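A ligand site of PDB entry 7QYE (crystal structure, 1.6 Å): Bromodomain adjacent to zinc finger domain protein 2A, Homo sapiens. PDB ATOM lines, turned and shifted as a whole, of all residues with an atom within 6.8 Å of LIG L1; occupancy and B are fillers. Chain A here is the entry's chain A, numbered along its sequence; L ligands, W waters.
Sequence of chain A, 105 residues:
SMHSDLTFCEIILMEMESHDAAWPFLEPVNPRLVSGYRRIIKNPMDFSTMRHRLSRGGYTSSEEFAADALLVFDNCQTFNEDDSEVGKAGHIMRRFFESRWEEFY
Water W1 lies within hydrogen-bond range of an oxygen (O1) of LIG L1 (2.6 Å), the side-chain hydroxyl (OH) of Tyr 37 (2.6 Å) and the backbone NH (N) of Cys 76 (3.5 Å).
Water W6 bridges N of Asn 30 and N2 of LIG L1.
The backbone carbonyl oxygen (O) of Val 86 sits at hydrogen-bond distance from the side-chain sulfur (SG) of Cys 76, at 3.3 Å.
The side-chain amide nitrogen (ND2) of Asn 80 is in hydrogen-bond range of the backbone carbonyl oxygen (O) of Cys 76 (3.1 Å).
Merely in contact with LIG L1: Trp 23 (3.8 Å), Phe 25 (3.8 Å), Val 29 (3.6 Å), Leu 33 (3.6 Å), Val 34 (3.9 Å), Tyr 37 (3.6 Å), Phe 79 (3.5 Å) and Val 86 (3.7 Å).
Hydrophobic or aromatic side chains that line LIG L1: Trp 23, Pro 24, Phe 25, Val 29, Leu 33, Val 34, Tyr 37, Phe 79 and Val 86.
Within 4 Å of LIG L1: Trp 23, Pro 24, Phe 25, Val 29, Leu 33, Val 34, Tyr 37, Phe 79, Asn 80 and Val 86.
The nearest printed residue that does not touch LIG L1 is Glu 27 (4.7 Å).
The backbone carbonyl oxygen of Pro 24 lies within hydrogen-bond range of a nitrogen (N1) of LIG L1.
The side-chain amide nitrogen (ND2) of Asn 80 is in hydrogen-bond range of an oxygen (O1) of LIG L1, at 2.9 Å.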
ATOM      1  N   TRP A  23      -0.357  21.741   1.564  1.00  0.00           N
ATOM      2  CA  TRP A  23       0.340  22.889   0.981  1.00  0.00           C
ATOM      3  C   TRP A  23       0.849  23.924   1.995  1.00  0.00           C
ATOM      4  O   TRP A  23       1.957  24.446   1.782  1.00  0.00           O
ATOM      5  CB  TRP A  23      -0.569  23.513  -0.091  1.00  0.00           C
ATOM      6  CG  TRP A  23      -1.865  23.977   0.417  1.00  0.00           C
ATOM      7  CD1 TRP A  23      -3.019  23.250   0.510  1.00  0.00           C
ATOM      8  CD2 TRP A  23      -2.164  25.274   0.964  1.00  0.00           C
ATOM      9  NE1 TRP A  23      -4.009  24.003   1.072  1.00  0.00           N
ATOM     10  CE2 TRP A  23      -3.510  25.249   1.366  1.00  0.00           C
ATOM     11  CE3 TRP A  23      -1.409  26.432   1.158  1.00  0.00           C
ATOM     12  CZ2 TRP A  23      -4.139  26.347   1.942  1.00  0.00           C
ATOM     13  CZ3 TRP A  23      -2.037  27.521   1.738  1.00  0.00           C
ATOM     14  CH2 TRP A  23      -3.380  27.482   2.108  1.00  0.00           C
ATOM     15  N   PRO A  24       0.158  24.246   3.098  1.00  0.00           N
ATOM     16  CA  PRO A  24       0.740  25.240   4.024  1.00  0.00           C
ATOM     17  C   PRO A  24       2.010  24.752   4.704  1.00  0.00           C
ATOM     18  O   PRO A  24       2.763  25.577   5.212  1.00  0.00           O
ATOM     19  CB  PRO A  24      -0.365  25.455   5.069  1.00  0.00           C
ATOM     20  CG  PRO A  24      -1.601  24.929   4.440  1.00  0.00           C
ATOM     21  CD  PRO A  24      -1.162  23.812   3.591  1.00  0.00           C
ATOM     22  N   PHE A  25       2.222  23.445   4.764  1.00  0.00           N
ATOM     23  CA  PHE A  25       3.197  22.868   5.677  1.00  0.00           C
ATOM     24  C   PHE A  25       4.403  22.269   4.974  1.00  0.00           C
ATOM     25  O   PHE A  25       5.281  21.714   5.650  1.00  0.00           O
ATOM     26  CB  PHE A  25       2.500  21.808   6.550  1.00  0.00           C
ATOM     27  CG  PHE A  25       1.193  22.278   7.100  1.00  0.00           C
ATOM     28  CD1 PHE A  25       1.159  23.257   8.083  1.00  0.00           C
ATOM     29  CD2 PHE A  25      -0.011  21.762   6.628  1.00  0.00           C
ATOM     30  CE1 PHE A  25      -0.055  23.713   8.596  1.00  0.00           C
ATOM     31  CE2 PHE A  25      -1.215  22.207   7.141  1.00  0.00           C
ATOM     32  CZ  PHE A  25      -1.242  23.194   8.115  1.00  0.00           C
ATOM     33  N   LEU A  26       4.507  22.398   3.655  1.00  0.00           N
ATOM     34  CA  LEU A  26       5.586  21.726   2.928  1.00  0.00           C
ATOM     35  C   LEU A  26       6.957  22.289   3.256  1.00  0.00           C
ATOM     36  O   LEU A  26       7.937  21.544   3.270  1.00  0.00           O
ATOM     37  CB  LEU A  26       5.344  21.816   1.432  1.00  0.00           C
ATOM     38  CG  LEU A  26       4.029  21.155   1.017  1.00  0.00           C
ATOM     39  CD1 LEU A  26       3.827  21.294  -0.479  1.00  0.00           C
ATOM     40  CD2 LEU A  26       4.036  19.708   1.439  1.00  0.00           C
ATOM     41  N   GLU A  27       7.062  23.589   3.495  1.00  0.00           N
ATOM     42  CA  GLU A  27       8.311  24.287   3.722  1.00  0.00           C
ATOM     43  C   GLU A  27       8.153  25.217   4.926  1.00  0.00           C
ATOM     44  O   GLU A  27       7.024  25.495   5.340  1.00  0.00           O
ATOM     45  CB  GLU A  27       8.703  25.095   2.463  1.00  0.00           C
ATOM     46  CG  GLU A  27       8.883  24.229   1.223  1.00  0.00           C
ATOM     47  CD  GLU A  27       9.618  24.937   0.103  1.00  0.00           C
ATOM     48  OE1 GLU A  27      10.683  24.436  -0.318  1.00  0.00           O
ATOM     49  OE2 GLU A  27       9.144  26.004  -0.352  1.00  0.00           O
ATOM     50  N   PRO A  28       9.267  25.697   5.513  1.00  0.00           N
ATOM     51  CA  PRO A  28       9.136  26.565   6.696  1.00  0.00           C
ATOM     52  C   PRO A  28       8.241  27.762   6.408  1.00  0.00           C
ATOM     53  O   PRO A  28       8.161  28.253   5.280  1.00  0.00           O
ATOM     54  CB  PRO A  28      10.576  27.011   6.967  1.00  0.00           C
ATOM     55  CG  PRO A  28      11.433  25.973   6.332  1.00  0.00           C
ATOM     56  CD  PRO A  28      10.673  25.459   5.151  1.00  0.00           C
ATOM     57  N   VAL A  29       7.547  28.245   7.452  1.00  0.00           N
ATOM     58  CA  VAL A  29       6.701  29.421   7.275  1.00  0.00           C
ATOM     59  C   VAL A  29       7.564  30.587   6.800  1.00  0.00           C
ATOM     60  O   VAL A  29       8.628  30.859   7.362  1.00  0.00           O
ATOM     61  CB  VAL A  29       5.937  29.756   8.574  1.00  0.00           C
ATOM     62  CG1 VAL A  29       5.158  31.057   8.430  1.00  0.00           C
ATOM     63  CG2 VAL A  29       4.976  28.624   8.910  1.00  0.00           C
ATOM     64  N   ASN A  30       7.122  31.244   5.730  1.00  0.00           N
ATOM     65  CA  ASN A  30       7.970  32.110   4.920  1.00  0.00           C
ATOM     66  C   ASN A  30       7.832  33.565   5.331  1.00  0.00           C
ATOM     67  O   ASN A  30       6.742  34.130   5.199  1.00  0.00           O
ATOM     68  CB  ASN A  30       7.584  31.936   3.450  1.00  0.00           C
ATOM     69  CG  ASN A  30       8.559  32.591   2.480  1.00  0.00           C
ATOM     70  OD1 ASN A  30       9.393  33.417   2.845  1.00  0.00           O
ATOM     71  ND2 ASN A  30       8.421  32.229   1.204  1.00  0.00           N
ATOM     72  N   LEU A  33       6.135  36.100   3.126  1.00  0.00           N
ATOM     73  CA  LEU A  33       4.695  36.034   2.959  1.00  0.00           C
ATOM     74  C   LEU A  33       3.909  36.473   4.176  1.00  0.00           C
ATOM     75  O   LEU A  33       2.708  36.739   4.056  1.00  0.00           O
ATOM     76  CB  LEU A  33       4.263  34.612   2.576  1.00  0.00           C
ATOM     77  CG  LEU A  33       4.847  34.040   1.274  1.00  0.00           C
ATOM     78  CD1 LEU A  33       4.380  32.611   1.033  1.00  0.00           C
ATOM     79  CD2 LEU A  33       4.546  34.916   0.060  1.00  0.00           C
ATOM     80  N   VAL A  34       4.532  36.524   5.356  1.00  0.00           N
ATOM     81  CA  VAL A  34       3.817  36.843   6.581  1.00  0.00           C
ATOM     82  C   VAL A  34       4.833  37.313   7.611  1.00  0.00           C
ATOM     83  O   VAL A  34       5.946  36.772   7.716  1.00  0.00           O
ATOM     84  CB  VAL A  34       3.013  35.614   7.093  1.00  0.00           C
ATOM     85  CG1 VAL A  34       3.969  34.499   7.492  1.00  0.00           C
ATOM     86  CG2 VAL A  34       2.120  36.021   8.250  1.00  0.00           C
ATOM     87  N   TYR A  37       5.763  35.895  12.602  1.00  0.00           N
ATOM     88  CA  TYR A  37       5.523  34.484  12.886  1.00  0.00           C
ATOM     89  C   TYR A  37       6.454  33.970  13.974  1.00  0.00           C
ATOM     90  O   TYR A  37       6.004  33.469  15.024  1.00  0.00           O
ATOM     91  CB  TYR A  37       5.682  33.650  11.602  1.00  0.00           C
ATOM     92  CG  TYR A  37       5.320  32.201  11.840  1.00  0.00           C
ATOM     93  CD1 TYR A  37       3.991  31.811  11.898  1.00  0.00           C
ATOM     94  CD2 TYR A  37       6.315  31.248  12.048  1.00  0.00           C
ATOM     95  CE1 TYR A  37       3.646  30.486  12.161  1.00  0.00           C
ATOM     96  CE2 TYR A  37       5.970  29.924  12.311  1.00  0.00           C
ATOM     97  CZ  TYR A  37       4.638  29.560  12.357  1.00  0.00           C
ATOM     98  OH  TYR A  37       4.285  28.250  12.604  1.00  0.00           O
ATOM     99  N   ILE A  41       5.921  32.035  17.458  1.00  0.00           N
ATOM    100  CA  ILE A  41       6.145  30.592  17.364  1.00  0.00           C
ATOM    101  C   ILE A  41       7.615  30.321  17.656  1.00  0.00           C
ATOM    102  O   ILE A  41       8.489  30.654  16.862  1.00  0.00           O
ATOM    103  CB  ILE A  41       5.732  30.077  15.979  1.00  0.00           C
ATOM    104  CG1 ILE A  41       4.243  30.357  15.733  1.00  0.00           C
ATOM    105  CG2 ILE A  41       6.029  28.608  15.854  1.00  0.00           C
ATOM    106  CD1 ILE A  41       3.310  29.785  16.800  1.00  0.00           C
ATOM    107  N   MET A  45       8.223  24.316  12.606  1.00  0.00           N
ATOM    108  CA  MET A  45       8.420  22.990  12.049  1.00  0.00           C
ATOM    109  C   MET A  45       7.603  22.875  10.764  1.00  0.00           C
ATOM    110  O   MET A  45       6.522  23.448  10.648  1.00  0.00           O
ATOM    111  CB  MET A  45       8.037  21.910  13.074  1.00  0.00           C
ATOM    112  CG  MET A  45       8.391  20.468  12.677  1.00  0.00           C
ATOM    113  SD  MET A  45      10.095  20.271  12.119  1.00  0.00           S
ATOM    114  CE  MET A  45      11.001  20.902  13.534  1.00  0.00           C
ATOM    115  N   VAL A  72       4.078  20.788  14.025  1.00  0.00           N
ATOM    116  CA  VAL A  72       3.536  21.484  12.853  1.00  0.00           C
ATOM    117  C   VAL A  72       2.093  21.912  13.108  1.00  0.00           C
ATOM    118  O   VAL A  72       1.693  23.076  12.867  1.00  0.00           O
ATOM    119  CB  VAL A  72       3.627  20.600  11.601  1.00  0.00           C
ATOM    120  CG1 VAL A  72       2.937  21.298  10.430  1.00  0.00           C
ATOM    121  CG2 VAL A  72       5.071  20.310  11.257  1.00  0.00           C
ATOM    122  N   ASN A  75       1.678  24.516  16.227  1.00  0.00           N
ATOM    123  CA  ASN A  75       2.033  25.856  15.753  1.00  0.00           C
ATOM    124  C   ASN A  75       0.902  26.434  14.912  1.00  0.00           C
ATOM    125  O   ASN A  75       0.521  27.598  15.074  1.00  0.00           O
ATOM    126  CB  ASN A  75       3.323  25.807  14.919  1.00  0.00           C
ATOM    127  CG  ASN A  75       4.556  25.502  15.742  1.00  0.00           C
ATOM    128  OD1 ASN A  75       4.543  25.608  16.967  1.00  0.00           O
ATOM    129  ND2 ASN A  75       5.657  25.136  15.070  1.00  0.00           N
ATOM    130  N   CYS A  76       0.387  25.635  13.980  1.00  0.00           N
ATOM    131  CA  CYS A  76      -0.658  26.112  13.088  1.00  0.00           C
ATOM    132  C   CYS A  76      -1.879  26.580  13.872  1.00  0.00           C
ATOM    133  O   CYS A  76      -2.423  27.655  13.600  1.00  0.00           O
ATOM    134  CB  CYS A  76      -1.034  25.028  12.095  1.00  0.00           C
ATOM    135  SG  CYS A  76      -2.267  25.530  10.903  1.00  0.00           S
ATOM    136  N   PHE A  79      -1.059  30.029  15.727  1.00  0.00           N
ATOM    137  CA  PHE A  79      -0.917  31.296  15.012  1.00  0.00           C
ATOM    138  C   PHE A  79      -2.129  31.683  14.169  1.00  0.00           C
ATOM    139  O   PHE A  79      -2.362  32.881  13.973  1.00  0.00           O
ATOM    140  CB  PHE A  79       0.314  31.233  14.117  1.00  0.00           C
ATOM    141  CG  PHE A  79       0.711  32.553  13.538  1.00  0.00           C
ATOM    142  CD1 PHE A  79       1.561  33.400  14.233  1.00  0.00           C
ATOM    143  CD2 PHE A  79       0.262  32.936  12.310  1.00  0.00           C
ATOM    144  CE1 PHE A  79       1.939  34.628  13.702  1.00  0.00           C
ATOM    145  CE2 PHE A  79       0.644  34.168  11.762  1.00  0.00           C
ATOM    146  CZ  PHE A  79       1.477  35.008  12.471  1.00  0.00           C
ATOM    147  N   ASN A  80      -2.886  30.714  13.664  1.00  0.00           N
ATOM    148  CA  ASN A  80      -3.926  30.945  12.669  1.00  0.00           C
ATOM    149  C   ASN A  80      -5.320  30.769  13.262  1.00  0.00           C
ATOM    150  O   ASN A  80      -5.542  29.911  14.117  1.00  0.00           O
ATOM    151  CB  ASN A  80      -3.778  29.985  11.474  1.00  0.00           C
ATOM    152  CG  ASN A  80      -2.440  30.123  10.767  1.00  0.00           C
ATOM    153  OD1 ASN A  80      -2.281  30.970   9.906  1.00  0.00           O
ATOM    154  ND2 ASN A  80      -1.490  29.264  11.122  1.00  0.00           N
ATOM    155  N   VAL A  86      -5.332  28.197   6.115  1.00  0.00           N
ATOM    156  CA  VAL A  86      -4.240  27.457   6.758  1.00  0.00           C
ATOM    157  C   VAL A  86      -4.719  26.781   8.039  1.00  0.00           C
ATOM    158  O   VAL A  86      -4.336  25.646   8.327  1.00  0.00           O
ATOM    159  CB  VAL A  86      -3.047  28.396   7.019  1.00  0.00           C
ATOM    160  CG1 VAL A  86      -1.984  27.695   7.827  1.00  0.00           C
ATOM    161  CG2 VAL A  86      -2.469  28.863   5.711  1.00  0.00           C
HETATM  162  C1  LIG L   1       1.460  31.599   9.349  1.00  0.00           C
HETATM  163  C2  LIG L   1       1.289  30.114   8.992  1.00  0.00           C
HETATM  164  C3  LIG L   1       1.400  29.573   7.540  1.00  0.00           C
HETATM  165  C4  LIG L   1       1.637  28.209   7.225  1.00  0.00           C
HETATM  166  C5  LIG L   1       1.828  27.010   8.229  1.00  0.00           C
HETATM  167  C6  LIG L   1       1.474  29.303   5.287  1.00  0.00           C
HETATM  168  C7  LIG L   1       1.295  30.267   6.303  1.00  0.00           C
HETATM  169  C8  LIG L   1       1.003  31.834   6.086  1.00  0.00           C
HETATM  170  C9  LIG L   1       1.984  32.399   4.941  1.00  0.00           C
HETATM  171  C10 LIG L   1       1.103  33.496   4.167  1.00  0.00           C
HETATM  172  C11 LIG L   1      -0.075  33.624   4.875  1.00  0.00           C
HETATM  173  C12 LIG L   1      -0.262  32.195   5.708  1.00  0.00           C
HETATM  174  C13 LIG L   1       1.426  29.448   3.755  1.00  0.00           C
HETATM  175  C14 LIG L   1       0.474  30.184   3.014  1.00  0.00           C
HETATM  176  C15 LIG L   1       2.070  29.033   1.522  1.00  0.00           C
HETATM  177  C16 LIG L   1       2.563  28.473  -1.031  1.00  0.00           C
HETATM  178  C17 LIG L   1       3.632  29.184  -1.907  1.00  0.00           C
HETATM  179  C18 LIG L   1       5.342  28.774  -0.298  1.00  0.00           C
HETATM  180  C19 LIG L   1       4.342  28.048   0.622  1.00  0.00           C
HETATM  181  N1  LIG L   1       1.669  28.089   5.892  1.00  0.00           N
HETATM  182  N2  LIG L   1       2.375  28.768   2.880  1.00  0.00           N
HETATM  183  N3  LIG L   1       2.922  28.533   0.415  1.00  0.00           N
HETATM  184  N4  LIG L   1       4.956  28.692  -1.663  1.00  0.00           N
HETATM  185  O1  LIG L   1       1.075  29.350   9.881  1.00  0.00           O
HETATM  186  S1  LIG L   1       0.790  30.046   1.409  1.00  0.00           S
HETATM  187  C1  LG2 L   2       1.568  31.780  -3.915  1.00  0.00           C
HETATM  188  C2  LG2 L   2       1.580  32.222  -2.448  1.00  0.00           C
HETATM  189  C3  LG2 L   2       0.258  32.193  -1.654  1.00  0.00           C
HETATM  190  C4  LG2 L   2      -0.125  33.105  -0.663  1.00  0.00           C
HETATM  191  C5  LG2 L   2       0.702  34.341  -0.153  1.00  0.00           C
HETATM  192  C6  LG2 L   2      -1.770  31.616  -0.873  1.00  0.00           C
HETATM  193  C7  LG2 L   2      -0.760  31.269  -1.812  1.00  0.00           C
HETATM  194  C8  LG2 L   2      -0.677  30.046  -2.861  1.00  0.00           C
HETATM  195  C9  LG2 L   2      -2.051  30.014  -3.698  1.00  0.00           C
HETATM  196  C10 LG2 L   2      -2.463  28.464  -3.712  1.00  0.00           C
HETATM  197  C11 LG2 L   2      -1.291  27.794  -3.496  1.00  0.00           C
HETATM  198  C12 LG2 L   2      -0.405  28.763  -2.475  1.00  0.00           C
HETATM  199  C13 LG2 L   2      -3.142  31.010  -0.619  1.00  0.00           C
HETATM  200  C14 LG2 L   2      -3.923  31.137   0.570  1.00  0.00           C
HETATM  201  C15 LG2 L   2      -5.164  29.859  -1.140  1.00  0.00           C
HETATM  202  C16 LG2 L   2      -7.615  29.177  -1.909  1.00  0.00           C
HETATM  203  C17 LG2 L   2      -8.227  29.451  -3.301  1.00  0.00           C
HETATM  204  C18 LG2 L   2      -6.888  27.542  -3.879  1.00  0.00           C
HETATM  205  C19 LG2 L   2      -5.709  28.075  -3.024  1.00  0.00           C
HETATM  206  N1  LG2 L   2      -1.341  32.749  -0.226  1.00  0.00           N
HETATM  207  N2  LG2 L   2      -3.899  30.267  -1.623  1.00  0.00           N
HETATM  208  N3  LG2 L   2      -6.126  29.069  -1.965  1.00  0.00           N
HETATM  209  N4  LG2 L   2      -7.830  28.524  -4.306  1.00  0.00           N
HETATM  210  O1  LG2 L   2       2.578  32.613  -1.947  1.00  0.00           O
HETATM  211  S1  LG2 L   2      -5.362  30.387   0.386  1.00  0.00           S
HETATM  212  O   HOH W   1       1.949  27.636  11.635  1.00  0.00           O
HETATM  213  O   HOH W   2       6.035  27.826   3.517  1.00  0.00           O
HETATM  214  O   HOH W   3       2.687  25.247  -1.090  1.00  0.00           O
HETATM  215  O   HOH W   4       5.801  25.195  -0.115  1.00  0.00           O
HETATM  216  O   HOH W   5       4.769  25.361   2.588  1.00  0.00           O
HETATM  217  O   HOH W   6       4.920  30.107   4.208  1.00  0.00           O
